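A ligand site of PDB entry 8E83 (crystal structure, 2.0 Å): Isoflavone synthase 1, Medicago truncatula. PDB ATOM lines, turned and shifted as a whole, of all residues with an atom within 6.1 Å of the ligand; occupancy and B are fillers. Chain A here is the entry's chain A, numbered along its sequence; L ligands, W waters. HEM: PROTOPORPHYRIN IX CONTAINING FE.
The side-chain sulfur (SG) of Cys 426 sits close to the backbone NH (N) of Gly 428 (3.1 Å). The side-chain sulfur of Cys 426 sits close to the backbone NH of Val 429, 3.1 Å away. O of Met 167 lies within hydrogen-bond range of N of Phe 249. The side-chain carboxylate (OD2) of Asp 277 lies within hydrogen-bond range of the indole nitrogen (NE1) of Trp 105.
An iron atom (FE) of the ligand is bound by the side-chain sulfur of Cys 426. The guanidinium group of Arg 423 is in salt-bridge range of an oxygen (O1D) of the ligand (2.7 Å). An oxygen (O1A) of the ligand is in salt-bridge range of the guanidinium group (NH1) of Arg 410, at 2.8 Å.
Water W4 lies within hydrogen-bond range of O2A of the ligand (2.7 Å), O of Gly 282 (2.8 Å) and OG1 of Thr 286 (2.8 Å). Water W1 lies within hydrogen-bond range of O2D of the ligand (2.9 Å), N of Leu 417 (3.0 Å) and N of Leu 416 (3.4 Å). Water W3 lies within hydrogen-bond range of the guanidinium group of Arg 410 (2.7 Å) and an oxygen (O2A) of the ligand (3.1 Å). Water W2 lies within hydrogen-bond range of O of Phe 278 (2.7 Å), N of Ala 281 (2.8 Å), OG1 of Thr 283 (2.9 Å) and O of Phe 279 (3.4 Å).
Residues that only touch the ligand: Ser 421 (3.1 Å), Phe 249 (3.1 Å), Phe 278 (3.3 Å), Thr 415 (3.3 Å), Gly 422 (3.4 Å), Ala 281 (3.4 Å), Ile 164 (3.6 Å), Gly 428 (3.6 Å), Leu 417 (3.6 Å), Val 429 (3.6 Å), Trp 105 (3.6 Å), Val 96 (3.7 Å), Pro 427 (3.7 Å), Ile 108 (3.7 Å), Thr 283 (3.8 Å), Ala 432 (3.8 Å), Ile 112 (3.8 Å), Leu 117 (3.9 Å), Ser 285 (3.9 Å) and Gly 282 (3.9 Å). Hydrophobic or aromatic side chains within 4 Å of the ligand: Val 96, Trp 105, Ile 108, Ile 112, Leu 117, Ile 164, Phe 249, Phe 278, Ala 281, Leu 417, Pro 427, Val 429 and Ala 432. Of the 33 residues printed, 23 come within 4 Å of the ligand. The nearest printed residue that does not touch the ligand is Met 168 (4.1 Å).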
ATOM      1  N   VAL A  96      18.080  35.730   1.522  1.00  0.00           N
ATOM      2  CA  VAL A  96      18.546  34.538   2.238  1.00  0.00           C
ATOM      3  C   VAL A  96      19.340  34.933   3.469  1.00  0.00           C
ATOM      4  O   VAL A  96      19.312  34.242   4.487  1.00  0.00           O
ATOM      5  CB  VAL A  96      19.367  33.630   1.288  1.00  0.00           C
ATOM      6  CG1 VAL A  96      19.865  32.400   2.041  1.00  0.00           C
ATOM      7  CG2 VAL A  96      18.532  33.209   0.096  1.00  0.00           C
ATOM      8  N   VAL A  99      17.835  34.885   7.048  1.00  0.00           N
ATOM      9  CA  VAL A  99      17.695  33.674   7.868  1.00  0.00           C
ATOM     10  C   VAL A  99      18.600  33.691   9.093  1.00  0.00           C
ATOM     11  O   VAL A  99      18.099  33.496  10.204  1.00  0.00           O
ATOM     12  CB  VAL A  99      17.889  32.417   6.991  1.00  0.00           C
ATOM     13  CG1 VAL A  99      17.879  31.173   7.861  1.00  0.00           C
ATOM     14  CG2 VAL A  99      16.803  32.338   5.925  1.00  0.00           C
ATOM     15  N   TRP A 105      12.994  36.392  12.044  1.00  0.00           N
ATOM     16  CA  TRP A 105      13.170  35.007  11.625  1.00  0.00           C
ATOM     17  C   TRP A 105      13.412  34.078  12.805  1.00  0.00           C
ATOM     18  O   TRP A 105      13.413  32.851  12.616  1.00  0.00           O
ATOM     19  CB  TRP A 105      14.315  34.899  10.627  1.00  0.00           C
ATOM     20  CG  TRP A 105      13.881  35.144   9.212  1.00  0.00           C
ATOM     21  CD1 TRP A 105      13.662  36.356   8.627  1.00  0.00           C
ATOM     22  CD2 TRP A 105      13.616  34.155   8.213  1.00  0.00           C
ATOM     23  NE1 TRP A 105      13.270  36.184   7.326  1.00  0.00           N
ATOM     24  CE2 TRP A 105      13.234  34.834   7.041  1.00  0.00           C
ATOM     25  CE3 TRP A 105      13.671  32.755   8.199  1.00  0.00           C
ATOM     26  CZ2 TRP A 105      12.909  34.171   5.865  1.00  0.00           C
ATOM     27  CZ3 TRP A 105      13.337  32.093   7.026  1.00  0.00           C
ATOM     28  CH2 TRP A 105      12.962  32.807   5.879  1.00  0.00           C
ATOM     29  N   ILE A 108      10.553  31.729  12.922  1.00  0.00           N
ATOM     30  CA  ILE A 108      10.673  30.565  12.052  1.00  0.00           C
ATOM     31  C   ILE A 108      11.537  29.492  12.712  1.00  0.00           C
ATOM     32  O   ILE A 108      11.218  28.305  12.647  1.00  0.00           O
ATOM     33  CB  ILE A 108      11.250  30.984  10.683  1.00  0.00           C
ATOM     34  CG1 ILE A 108      10.328  31.992   9.997  1.00  0.00           C
ATOM     35  CG2 ILE A 108      11.461  29.759   9.796  1.00  0.00           C
ATOM     36  CD1 ILE A 108       8.960  31.449   9.673  1.00  0.00           C
ATOM     37  N   ILE A 112      10.677  25.494  13.692  1.00  0.00           N
ATOM     38  CA  ILE A 112      11.474  24.375  13.209  1.00  0.00           C
ATOM     39  C   ILE A 112      11.919  23.494  14.369  1.00  0.00           C
ATOM     40  O   ILE A 112      11.775  22.267  14.329  1.00  0.00           O
ATOM     41  CB  ILE A 112      12.672  24.884  12.391  1.00  0.00           C
ATOM     42  CG1 ILE A 112      12.185  25.564  11.112  1.00  0.00           C
ATOM     43  CG2 ILE A 112      13.632  23.743  12.067  1.00  0.00           C
ATOM     44  CD1 ILE A 112      13.301  26.161  10.271  1.00  0.00           C
ATOM     45  N   LEU A 117       7.272  23.129  11.861  1.00  0.00           N
ATOM     46  CA  LEU A 117       7.594  23.388  10.466  1.00  0.00           C
ATOM     47  C   LEU A 117       8.728  22.456  10.075  1.00  0.00           C
ATOM     48  O   LEU A 117       9.816  22.538  10.653  1.00  0.00           O
ATOM     49  CB  LEU A 117       7.994  24.862  10.262  1.00  0.00           C
ATOM     50  CG  LEU A 117       8.517  25.264   8.885  1.00  0.00           C
ATOM     51  CD1 LEU A 117       7.498  24.920   7.815  1.00  0.00           C
ATOM     52  CD2 LEU A 117       8.836  26.750   8.865  1.00  0.00           C
ATOM     53  N   ILE A 164       5.964  29.816  -6.682  1.00  0.00           N
ATOM     54  CA  ILE A 164       6.340  30.429  -5.403  1.00  0.00           C
ATOM     55  C   ILE A 164       5.120  31.087  -4.760  1.00  0.00           C
ATOM     56  O   ILE A 164       4.828  30.873  -3.577  1.00  0.00           O
ATOM     57  CB  ILE A 164       7.490  31.434  -5.609  1.00  0.00           C
ATOM     58  CG1 ILE A 164       8.813  30.692  -5.843  1.00  0.00           C
ATOM     59  CG2 ILE A 164       7.581  32.396  -4.426  1.00  0.00           C
ATOM     60  CD1 ILE A 164       9.164  29.705  -4.759  1.00  0.00           C
ATOM     61  N   MET A 167       2.375  28.373  -3.715  1.00  0.00           N
ATOM     62  CA  MET A 167       2.782  27.611  -2.534  1.00  0.00           C
ATOM     63  C   MET A 167       2.678  28.456  -1.280  1.00  0.00           C
ATOM     64  O   MET A 167       2.272  27.972  -0.218  1.00  0.00           O
ATOM     65  CB  MET A 167       4.213  27.109  -2.703  1.00  0.00           C
ATOM     66  CG  MET A 167       4.351  25.877  -3.591  1.00  0.00           C
ATOM     67  SD  MET A 167       6.005  25.171  -3.441  1.00  0.00           S
ATOM     68  CE  MET A 167       7.017  26.524  -4.052  1.00  0.00           C
ATOM     69  N   MET A 168       3.049  29.741  -1.383  1.00  0.00           N
ATOM     70  CA  MET A 168       3.065  30.617  -0.213  1.00  0.00           C
ATOM     71  C   MET A 168       1.663  31.047   0.189  1.00  0.00           C
ATOM     72  O   MET A 168       1.327  31.037   1.379  1.00  0.00           O
ATOM     73  CB  MET A 168       3.931  31.840  -0.518  1.00  0.00           C
ATOM     74  CG  MET A 168       4.132  32.781   0.650  1.00  0.00           C
ATOM     75  SD  MET A 168       4.706  34.392   0.090  1.00  0.00           S
ATOM     76  CE  MET A 168       5.857  33.917  -1.198  1.00  0.00           C
ATOM     77  N   PHE A 249       1.505  27.694   2.737  1.00  0.00           N
ATOM     78  CA  PHE A 249       2.599  27.832   3.695  1.00  0.00           C
ATOM     79  C   PHE A 249       2.283  28.901   4.744  1.00  0.00           C
ATOM     80  O   PHE A 249       2.575  28.711   5.926  1.00  0.00           O
ATOM     81  CB  PHE A 249       3.904  28.158   2.981  1.00  0.00           C
ATOM     82  CG  PHE A 249       5.134  27.909   3.806  1.00  0.00           C
ATOM     83  CD1 PHE A 249       5.816  26.708   3.704  1.00  0.00           C
ATOM     84  CD2 PHE A 249       5.581  28.857   4.712  1.00  0.00           C
ATOM     85  CE1 PHE A 249       6.944  26.472   4.467  1.00  0.00           C
ATOM     86  CE2 PHE A 249       6.719  28.621   5.472  1.00  0.00           C
ATOM     87  CZ  PHE A 249       7.396  27.434   5.352  1.00  0.00           C
ATOM     88  N   LEU A 253       2.339  29.525   9.342  1.00  0.00           N
ATOM     89  CA  LEU A 253       2.866  30.647  10.106  1.00  0.00           C
ATOM     90  C   LEU A 253       1.778  31.334  10.916  1.00  0.00           C
ATOM     91  O   LEU A 253       1.973  31.655  12.091  1.00  0.00           O
ATOM     92  CB  LEU A 253       3.537  31.650   9.164  1.00  0.00           C
ATOM     93  CG  LEU A 253       4.610  31.075   8.241  1.00  0.00           C
ATOM     94  CD1 LEU A 253       5.293  32.184   7.451  1.00  0.00           C
ATOM     95  CD2 LEU A 253       5.632  30.280   9.031  1.00  0.00           C
ATOM     96  N   ASP A 277      10.515  38.568   2.235  1.00  0.00           N
ATOM     97  CA  ASP A 277      11.706  37.725   2.150  1.00  0.00           C
ATOM     98  C   ASP A 277      11.444  36.490   1.286  1.00  0.00           C
ATOM     99  O   ASP A 277      12.329  36.041   0.548  1.00  0.00           O
ATOM    100  CB  ASP A 277      12.151  37.309   3.552  1.00  0.00           C
ATOM    101  CG  ASP A 277      12.586  38.492   4.397  1.00  0.00           C
ATOM    102  OD1 ASP A 277      12.877  39.563   3.835  1.00  0.00           O
ATOM    103  OD2 ASP A 277      12.645  38.338   5.644  1.00  0.00           O
ATOM    104  N   PHE A 278      10.228  35.934   1.371  1.00  0.00           N
ATOM    105  CA  PHE A 278       9.911  34.735   0.604  1.00  0.00           C
ATOM    106  C   PHE A 278       9.898  35.012  -0.900  1.00  0.00           C
ATOM    107  O   PHE A 278      10.190  34.105  -1.701  1.00  0.00           O
ATOM    108  CB  PHE A 278       8.558  34.164   1.034  1.00  0.00           C
ATOM    109  CG  PHE A 278       8.521  33.688   2.464  1.00  0.00           C
ATOM    110  CD1 PHE A 278       9.668  33.260   3.102  1.00  0.00           C
ATOM    111  CD2 PHE A 278       7.322  33.665   3.169  1.00  0.00           C
ATOM    112  CE1 PHE A 278       9.627  32.814   4.412  1.00  0.00           C
ATOM    113  CE2 PHE A 278       7.278  33.221   4.469  1.00  0.00           C
ATOM    114  CZ  PHE A 278       8.432  32.795   5.095  1.00  0.00           C
ATOM    115  N   PHE A 279       9.544  36.229  -1.306  1.00  0.00           N
ATOM    116  CA  PHE A 279       9.503  36.584  -2.723  1.00  0.00           C
ATOM    117  C   PHE A 279      10.858  37.006  -3.297  1.00  0.00           C
ATOM    118  O   PHE A 279      10.986  37.098  -4.516  1.00  0.00           O
ATOM    119  CB  PHE A 279       8.522  37.730  -2.964  1.00  0.00           C
ATOM    120  CG  PHE A 279       7.075  37.302  -3.053  1.00  0.00           C
ATOM    121  CD1 PHE A 279       6.658  36.416  -4.030  1.00  0.00           C
ATOM    122  CD2 PHE A 279       6.147  37.820  -2.173  1.00  0.00           C
ATOM    123  CE1 PHE A 279       5.336  36.035  -4.115  1.00  0.00           C
ATOM    124  CE2 PHE A 279       4.816  37.448  -2.254  1.00  0.00           C
ATOM    125  CZ  PHE A 279       4.411  36.550  -3.226  1.00  0.00           C
ATOM    126  N   ALA A 281      14.236  35.825  -2.573  1.00  0.00           N
ATOM    127  CA  ALA A 281      15.368  34.966  -2.262  1.00  0.00           C
ATOM    128  C   ALA A 281      16.043  34.398  -3.509  1.00  0.00           C
ATOM    129  O   ALA A 281      16.953  33.567  -3.381  1.00  0.00           O
ATOM    130  CB  ALA A 281      14.946  33.836  -1.332  1.00  0.00           C
ATOM    131  N   GLY A 282      15.630  34.816  -4.698  1.00  0.00           N
ATOM    132  CA  GLY A 282      16.260  34.335  -5.916  1.00  0.00           C
ATOM    133  C   GLY A 282      15.429  33.323  -6.675  1.00  0.00           C
ATOM    134  O   GLY A 282      15.959  32.326  -7.172  1.00  0.00           O
ATOM    135  N   THR A 283      14.117  33.569  -6.757  1.00  0.00           N
ATOM    136  CA  THR A 283      13.234  32.680  -7.510  1.00  0.00           C
ATOM    137  C   THR A 283      13.700  32.494  -8.944  1.00  0.00           C
ATOM    138  O   THR A 283      13.608  31.405  -9.504  1.00  0.00           O
ATOM    139  CB  THR A 283      11.803  33.235  -7.479  1.00  0.00           C
ATOM    140  OG1 THR A 283      11.335  33.294  -6.131  1.00  0.00           O
ATOM    141  CG2 THR A 283      10.866  32.370  -8.307  1.00  0.00           C
ATOM    142  N   ASP A 284      14.230  33.565  -9.546  1.00  0.00           N
ATOM    143  CA  ASP A 284      14.617  33.519 -10.952  1.00  0.00           C
ATOM    144  C   ASP A 284      15.779  32.565 -11.217  1.00  0.00           C
ATOM    145  O   ASP A 284      15.969  32.156 -12.365  1.00  0.00           O
ATOM    146  CB  ASP A 284      14.985  34.922 -11.446  1.00  0.00           C
ATOM    147  CG  ASP A 284      16.243  35.472 -10.791  1.00  0.00           C
ATOM    148  OD1 ASP A 284      16.449  35.220  -9.585  1.00  0.00           O
ATOM    149  OD2 ASP A 284      17.034  36.146 -11.490  1.00  0.00           O
ATOM    150  N   SER A 285      16.552  32.202 -10.180  1.00  0.00           N
ATOM    151  CA  SER A 285      17.648  31.259 -10.381  1.00  0.00           C
ATOM    152  C   SER A 285      17.139  29.926 -10.924  1.00  0.00           C
ATOM    153  O   SER A 285      17.800  29.299 -11.765  1.00  0.00           O
ATOM    154  CB  SER A 285      18.397  31.033  -9.068  1.00  0.00           C
ATOM    155  OG  SER A 285      19.209  32.161  -8.749  1.00  0.00           O
ATOM    156  N   THR A 286      15.983  29.476 -10.457  1.00  0.00           N
ATOM    157  CA  THR A 286      15.439  28.204 -10.936  1.00  0.00           C
ATOM    158  C   THR A 286      14.975  28.314 -12.387  1.00  0.00           C
ATOM    159  O   THR A 286      15.178  27.387 -13.176  1.00  0.00           O
ATOM    160  CB  THR A 286      14.298  27.759 -10.028  1.00  0.00           C
ATOM    161  OG1 THR A 286      14.826  27.459  -8.725  1.00  0.00           O
ATOM    162  CG2 THR A 286      13.602  26.507 -10.595  1.00  0.00           C
ATOM    163  N   ARG A 410      21.730  19.442  -7.162  1.00  0.00           N
ATOM    164  CA  ARG A 410      22.486  20.397  -7.959  1.00  0.00           C
ATOM    165  C   ARG A 410      23.992  20.191  -7.854  1.00  0.00           C
ATOM    166  O   ARG A 410      24.714  20.590  -8.772  1.00  0.00           O
ATOM    167  CB  ARG A 410      22.142  21.829  -7.545  1.00  0.00           C
ATOM    168  CG  ARG A 410      20.741  22.279  -7.913  1.00  0.00           C
ATOM    169  CD  ARG A 410      20.426  23.635  -7.299  1.00  0.00           C
ATOM    170  NE  ARG A 410      20.339  23.561  -5.835  1.00  0.00           N
ATOM    171  CZ  ARG A 410      20.274  24.613  -5.033  1.00  0.00           C
ATOM    172  NH1 ARG A 410      20.285  25.837  -5.547  1.00  0.00           N
ATOM    173  NH2 ARG A 410      20.195  24.443  -3.726  1.00  0.00           N
ATOM    174  N   THR A 415      25.911  23.936  -1.474  1.00  0.00           N
ATOM    175  CA  THR A 415      25.390  24.968  -0.592  1.00  0.00           C
ATOM    176  C   THR A 415      26.454  25.428   0.390  1.00  0.00           C
ATOM    177  O   THR A 415      27.333  24.656   0.772  1.00  0.00           O
ATOM    178  CB  THR A 415      24.160  24.487   0.188  1.00  0.00           C
ATOM    179  OG1 THR A 415      24.589  23.631   1.262  1.00  0.00           O
ATOM    180  CG2 THR A 415      23.237  23.696  -0.726  1.00  0.00           C
ATOM    181  N   LEU A 416      26.363  26.699   0.805  1.00  0.00           N
ATOM    182  CA  LEU A 416      27.325  27.273   1.732  1.00  0.00           C
ATOM    183  C   LEU A 416      26.778  27.456   3.137  1.00  0.00           C
ATOM    184  O   LEU A 416      27.562  27.658   4.071  1.00  0.00           O
ATOM    185  CB  LEU A 416      27.810  28.637   1.207  1.00  0.00           C
ATOM    186  N   LEU A 417      25.458  27.362   3.325  1.00  0.00           N
ATOM    187  CA  LEU A 417      24.876  27.551   4.646  1.00  0.00           C
ATOM    188  C   LEU A 417      25.047  26.295   5.491  1.00  0.00           C
ATOM    189  O   LEU A 417      24.991  25.176   4.978  1.00  0.00           O
ATOM    190  CB  LEU A 417      23.407  27.908   4.536  1.00  0.00           C
ATOM    191  CG  LEU A 417      23.120  29.406   4.372  1.00  0.00           C
ATOM    192  CD1 LEU A 417      21.706  29.631   3.841  1.00  0.00           C
ATOM    193  CD2 LEU A 417      23.307  30.140   5.688  1.00  0.00           C
ATOM    194  N   SER A 421      20.204  25.079   8.780  1.00  0.00           N
ATOM    195  CA  SER A 421      19.780  26.435   8.462  1.00  0.00           C
ATOM    196  C   SER A 421      18.327  26.507   8.000  1.00  0.00           C
ATOM    197  O   SER A 421      17.756  27.595   7.975  1.00  0.00           O
ATOM    198  CB  SER A 421      20.681  27.037   7.389  1.00  0.00           C
ATOM    199  OG  SER A 421      22.025  27.091   7.844  1.00  0.00           O
ATOM    200  N   GLY A 422      17.731  25.380   7.636  1.00  0.00           N
ATOM    201  CA  GLY A 422      16.342  25.327   7.239  1.00  0.00           C
ATOM    202  C   GLY A 422      16.074  24.975   5.783  1.00  0.00           C
ATOM    203  O   GLY A 422      14.952  25.180   5.319  1.00  0.00           O
ATOM    204  N   ARG A 423      17.074  24.457   5.072  1.00  0.00           N
ATOM    205  CA  ARG A 423      16.894  24.104   3.665  1.00  0.00           C
ATOM    206  C   ARG A 423      15.750  23.117   3.470  1.00  0.00           C
ATOM    207  O   ARG A 423      14.984  23.213   2.509  1.00  0.00           O
ATOM    208  CB  ARG A 423      18.185  23.534   3.090  1.00  0.00           C
ATOM    209  CG  ARG A 423      19.250  24.570   2.777  1.00  0.00           C
ATOM    210  CD  ARG A 423      20.523  23.896   2.274  1.00  0.00           C
ATOM    211  NE  ARG A 423      20.233  22.766   1.395  1.00  0.00           N
ATOM    212  CZ  ARG A 423      20.002  22.863   0.094  1.00  0.00           C
ATOM    213  NH1 ARG A 423      20.011  24.060  -0.499  1.00  0.00           N
ATOM    214  NH2 ARG A 423      19.748  21.786  -0.627  1.00  0.00           N
ATOM    215  N   MET A 425      13.010  22.805   5.009  1.00  0.00           N
ATOM    216  CA  MET A 425      11.690  23.374   5.242  1.00  0.00           C
ATOM    217  C   MET A 425      11.331  24.459   4.242  1.00  0.00           C
ATOM    218  O   MET A 425      10.295  25.106   4.382  1.00  0.00           O
ATOM    219  CB  MET A 425      11.599  23.936   6.662  1.00  0.00           C
ATOM    220  CG  MET A 425      11.819  22.920   7.759  1.00  0.00           C
ATOM    221  SD  MET A 425      13.555  22.571   8.066  1.00  0.00           S
ATOM    222  CE  MET A 425      13.407  21.229   9.235  1.00  0.00           C
ATOM    223  N   CYS A 426      12.175  24.667   3.231  1.00  0.00           N
ATOM    224  CA  CYS A 426      12.016  25.806   2.350  1.00  0.00           C
ATOM    225  C   CYS A 426      11.394  25.381   1.030  1.00  0.00           C
ATOM    226  O   CYS A 426      11.998  24.583   0.303  1.00  0.00           O
ATOM    227  CB  CYS A 426      13.367  26.468   2.096  1.00  0.00           C
ATOM    228  SG  CYS A 426      13.297  27.527   0.665  1.00  0.00           S
ATOM    229  N   PRO A 427      10.206  25.882   0.682  1.00  0.00           N
ATOM    230  CA  PRO A 427       9.627  25.545  -0.625  1.00  0.00           C
ATOM    231  C   PRO A 427      10.461  26.033  -1.793  1.00  0.00           C
ATOM    232  O   PRO A 427      10.392  25.439  -2.875  1.00  0.00           O
ATOM    233  CB  PRO A 427       8.258  26.240  -0.587  1.00  0.00           C
ATOM    234  CG  PRO A 427       7.964  26.467   0.866  1.00  0.00           C
ATOM    235  CD  PRO A 427       9.296  26.713   1.507  1.00  0.00           C
ATOM    236  N   GLY A 428      11.255  27.084  -1.609  1.00  0.00           N
ATOM    237  CA  GLY A 428      12.093  27.569  -2.695  1.00  0.00           C
ATOM    238  C   GLY A 428      13.237  26.635  -3.015  1.00  0.00           C
ATOM    239  O   GLY A 428      13.551  26.409  -4.188  1.00  0.00           O
ATOM    240  N   VAL A 429      13.887  26.084  -1.985  1.00  0.00           N
ATOM    241  CA  VAL A 429      14.925  25.076  -2.213  1.00  0.00           C
ATOM    242  C   VAL A 429      14.334  23.838  -2.883  1.00  0.00           C
ATOM    243  O   VAL A 429      14.970  23.214  -3.737  1.00  0.00           O
ATOM    244  CB  VAL A 429      15.617  24.727  -0.883  1.00  0.00           C
ATOM    245  CG1 VAL A 429      16.481  23.490  -1.047  1.00  0.00           C
ATOM    246  CG2 VAL A 429      16.462  25.900  -0.417  1.00  0.00           C
ATOM    247  N   ALA A 432      13.850  24.614  -6.507  1.00  0.00           N
ATOM    248  CA  ALA A 432      15.136  24.702  -7.195  1.00  0.00           C
ATOM    249  C   ALA A 432      15.806  23.344  -7.386  1.00  0.00           C
ATOM    250  O   ALA A 432      16.818  23.272  -8.094  1.00  0.00           O
ATOM    251  CB  ALA A 432      16.077  25.627  -6.421  1.00  0.00           C
HETATM  252  CHA HEM L   1      16.644  29.742  -0.247  1.00  0.00           C
HETATM  253  CHB HEM L   1      12.075  30.959  -1.328  1.00  0.00           C
HETATM  254  CHC HEM L   1      10.695  29.758   3.160  1.00  0.00           C
HETATM  255  CHD HEM L   1      15.305  28.760   4.321  1.00  0.00           C
HETATM  256  C1A HEM L   1      15.509  30.101  -0.954  1.00  0.00           C
HETATM  257  C2A HEM L   1      15.423  30.319  -2.394  1.00  0.00           C
HETATM  258  C3A HEM L   1      14.164  30.649  -2.677  1.00  0.00           C
HETATM  259  C4A HEM L   1      13.410  30.666  -1.452  1.00  0.00           C
HETATM  260  CMA HEM L   1      13.615  30.977  -4.085  1.00  0.00           C
HETATM  261  CAA HEM L   1      16.572  30.185  -3.419  1.00  0.00           C
HETATM  262  CBA HEM L   1      16.938  28.714  -3.550  1.00  0.00           C
HETATM  263  CGA HEM L   1      17.977  28.543  -4.633  1.00  0.00           C
HETATM  264  O1A HEM L   1      19.059  27.981  -4.328  1.00  0.00           O
HETATM  265  O2A HEM L   1      17.722  28.990  -5.780  1.00  0.00           O
HETATM  266  C1B HEM L   1      11.289  30.684  -0.230  1.00  0.00           C
HETATM  267  C2B HEM L   1       9.840  30.741  -0.188  1.00  0.00           C
HETATM  268  C3B HEM L   1       9.448  30.422   1.037  1.00  0.00           C
HETATM  269  C4B HEM L   1      10.639  30.138   1.836  1.00  0.00           C
HETATM  270  CMB HEM L   1       8.903  31.121  -1.354  1.00  0.00           C
HETATM  271  CAB HEM L   1       7.968  30.374   1.462  1.00  0.00           C
HETATM  272  CBB HEM L   1       7.586  30.210   2.733  1.00  0.00           C
HETATM  273  C1C HEM L   1      11.811  29.399   3.874  1.00  0.00           C
HETATM  274  C2C HEM L   1      11.845  29.018   5.267  1.00  0.00           C
HETATM  275  C3C HEM L   1      13.101  28.748   5.616  1.00  0.00           C
HETATM  276  C4C HEM L   1      13.934  28.936   4.425  1.00  0.00           C
HETATM  277  CMC HEM L   1      10.622  28.966   6.207  1.00  0.00           C
HETATM  278  CAC HEM L   1      13.519  28.311   7.032  1.00  0.00           C
HETATM  279  CBC HEM L   1      14.789  28.313   7.447  1.00  0.00           C
HETATM  280  C1D HEM L   1      16.059  28.921   3.181  1.00  0.00           C
HETATM  281  C2D HEM L   1      17.491  28.684   3.070  1.00  0.00           C
HETATM  282  C3D HEM L   1      17.863  28.958   1.810  1.00  0.00           C
HETATM  283  C4D HEM L   1      16.678  29.374   1.075  1.00  0.00           C
HETATM  284  CMD HEM L   1      18.422  28.207   4.209  1.00  0.00           C
HETATM  285  CAD HEM L   1      19.291  28.851   1.236  1.00  0.00           C
HETATM  286  CBD HEM L   1      19.526  27.475   0.632  1.00  0.00           C
HETATM  287  CGD HEM L   1      20.842  27.459  -0.105  1.00  0.00           C
HETATM  288  O1D HEM L   1      21.349  26.348  -0.404  1.00  0.00           O
HETATM  289  O2D HEM L   1      21.395  28.555  -0.381  1.00  0.00           O
HETATM  290  NA  HEM L   1      14.257  30.320  -0.412  1.00  0.00           N
HETATM  291  NB  HEM L   1      11.740  30.315   1.019  1.00  0.00           N
HETATM  292  NC  HEM L   1      13.111  29.339   3.399  1.00  0.00           N
HETATM  293  ND  HEM L   1      15.613  29.338   1.949  1.00  0.00           N
HETATM  294 FE   HEM L   1      13.692  29.905   1.526  1.00  0.00          FE
HETATM  295  O   HOH W   1      23.787  28.814   1.301  1.00  0.00           O
HETATM  296  O   HOH W   2      12.221  34.076  -3.438  1.00  0.00           O
HETATM  297  O   HOH W   3      19.981  27.715  -7.396  1.00  0.00           O
HETATM  298  O   HOH W   4      15.459  29.610  -7.108  1.00  0.00           O
HETATM  299  O   HOH W   5      14.046  32.300   2.179  1.00  0.00           O
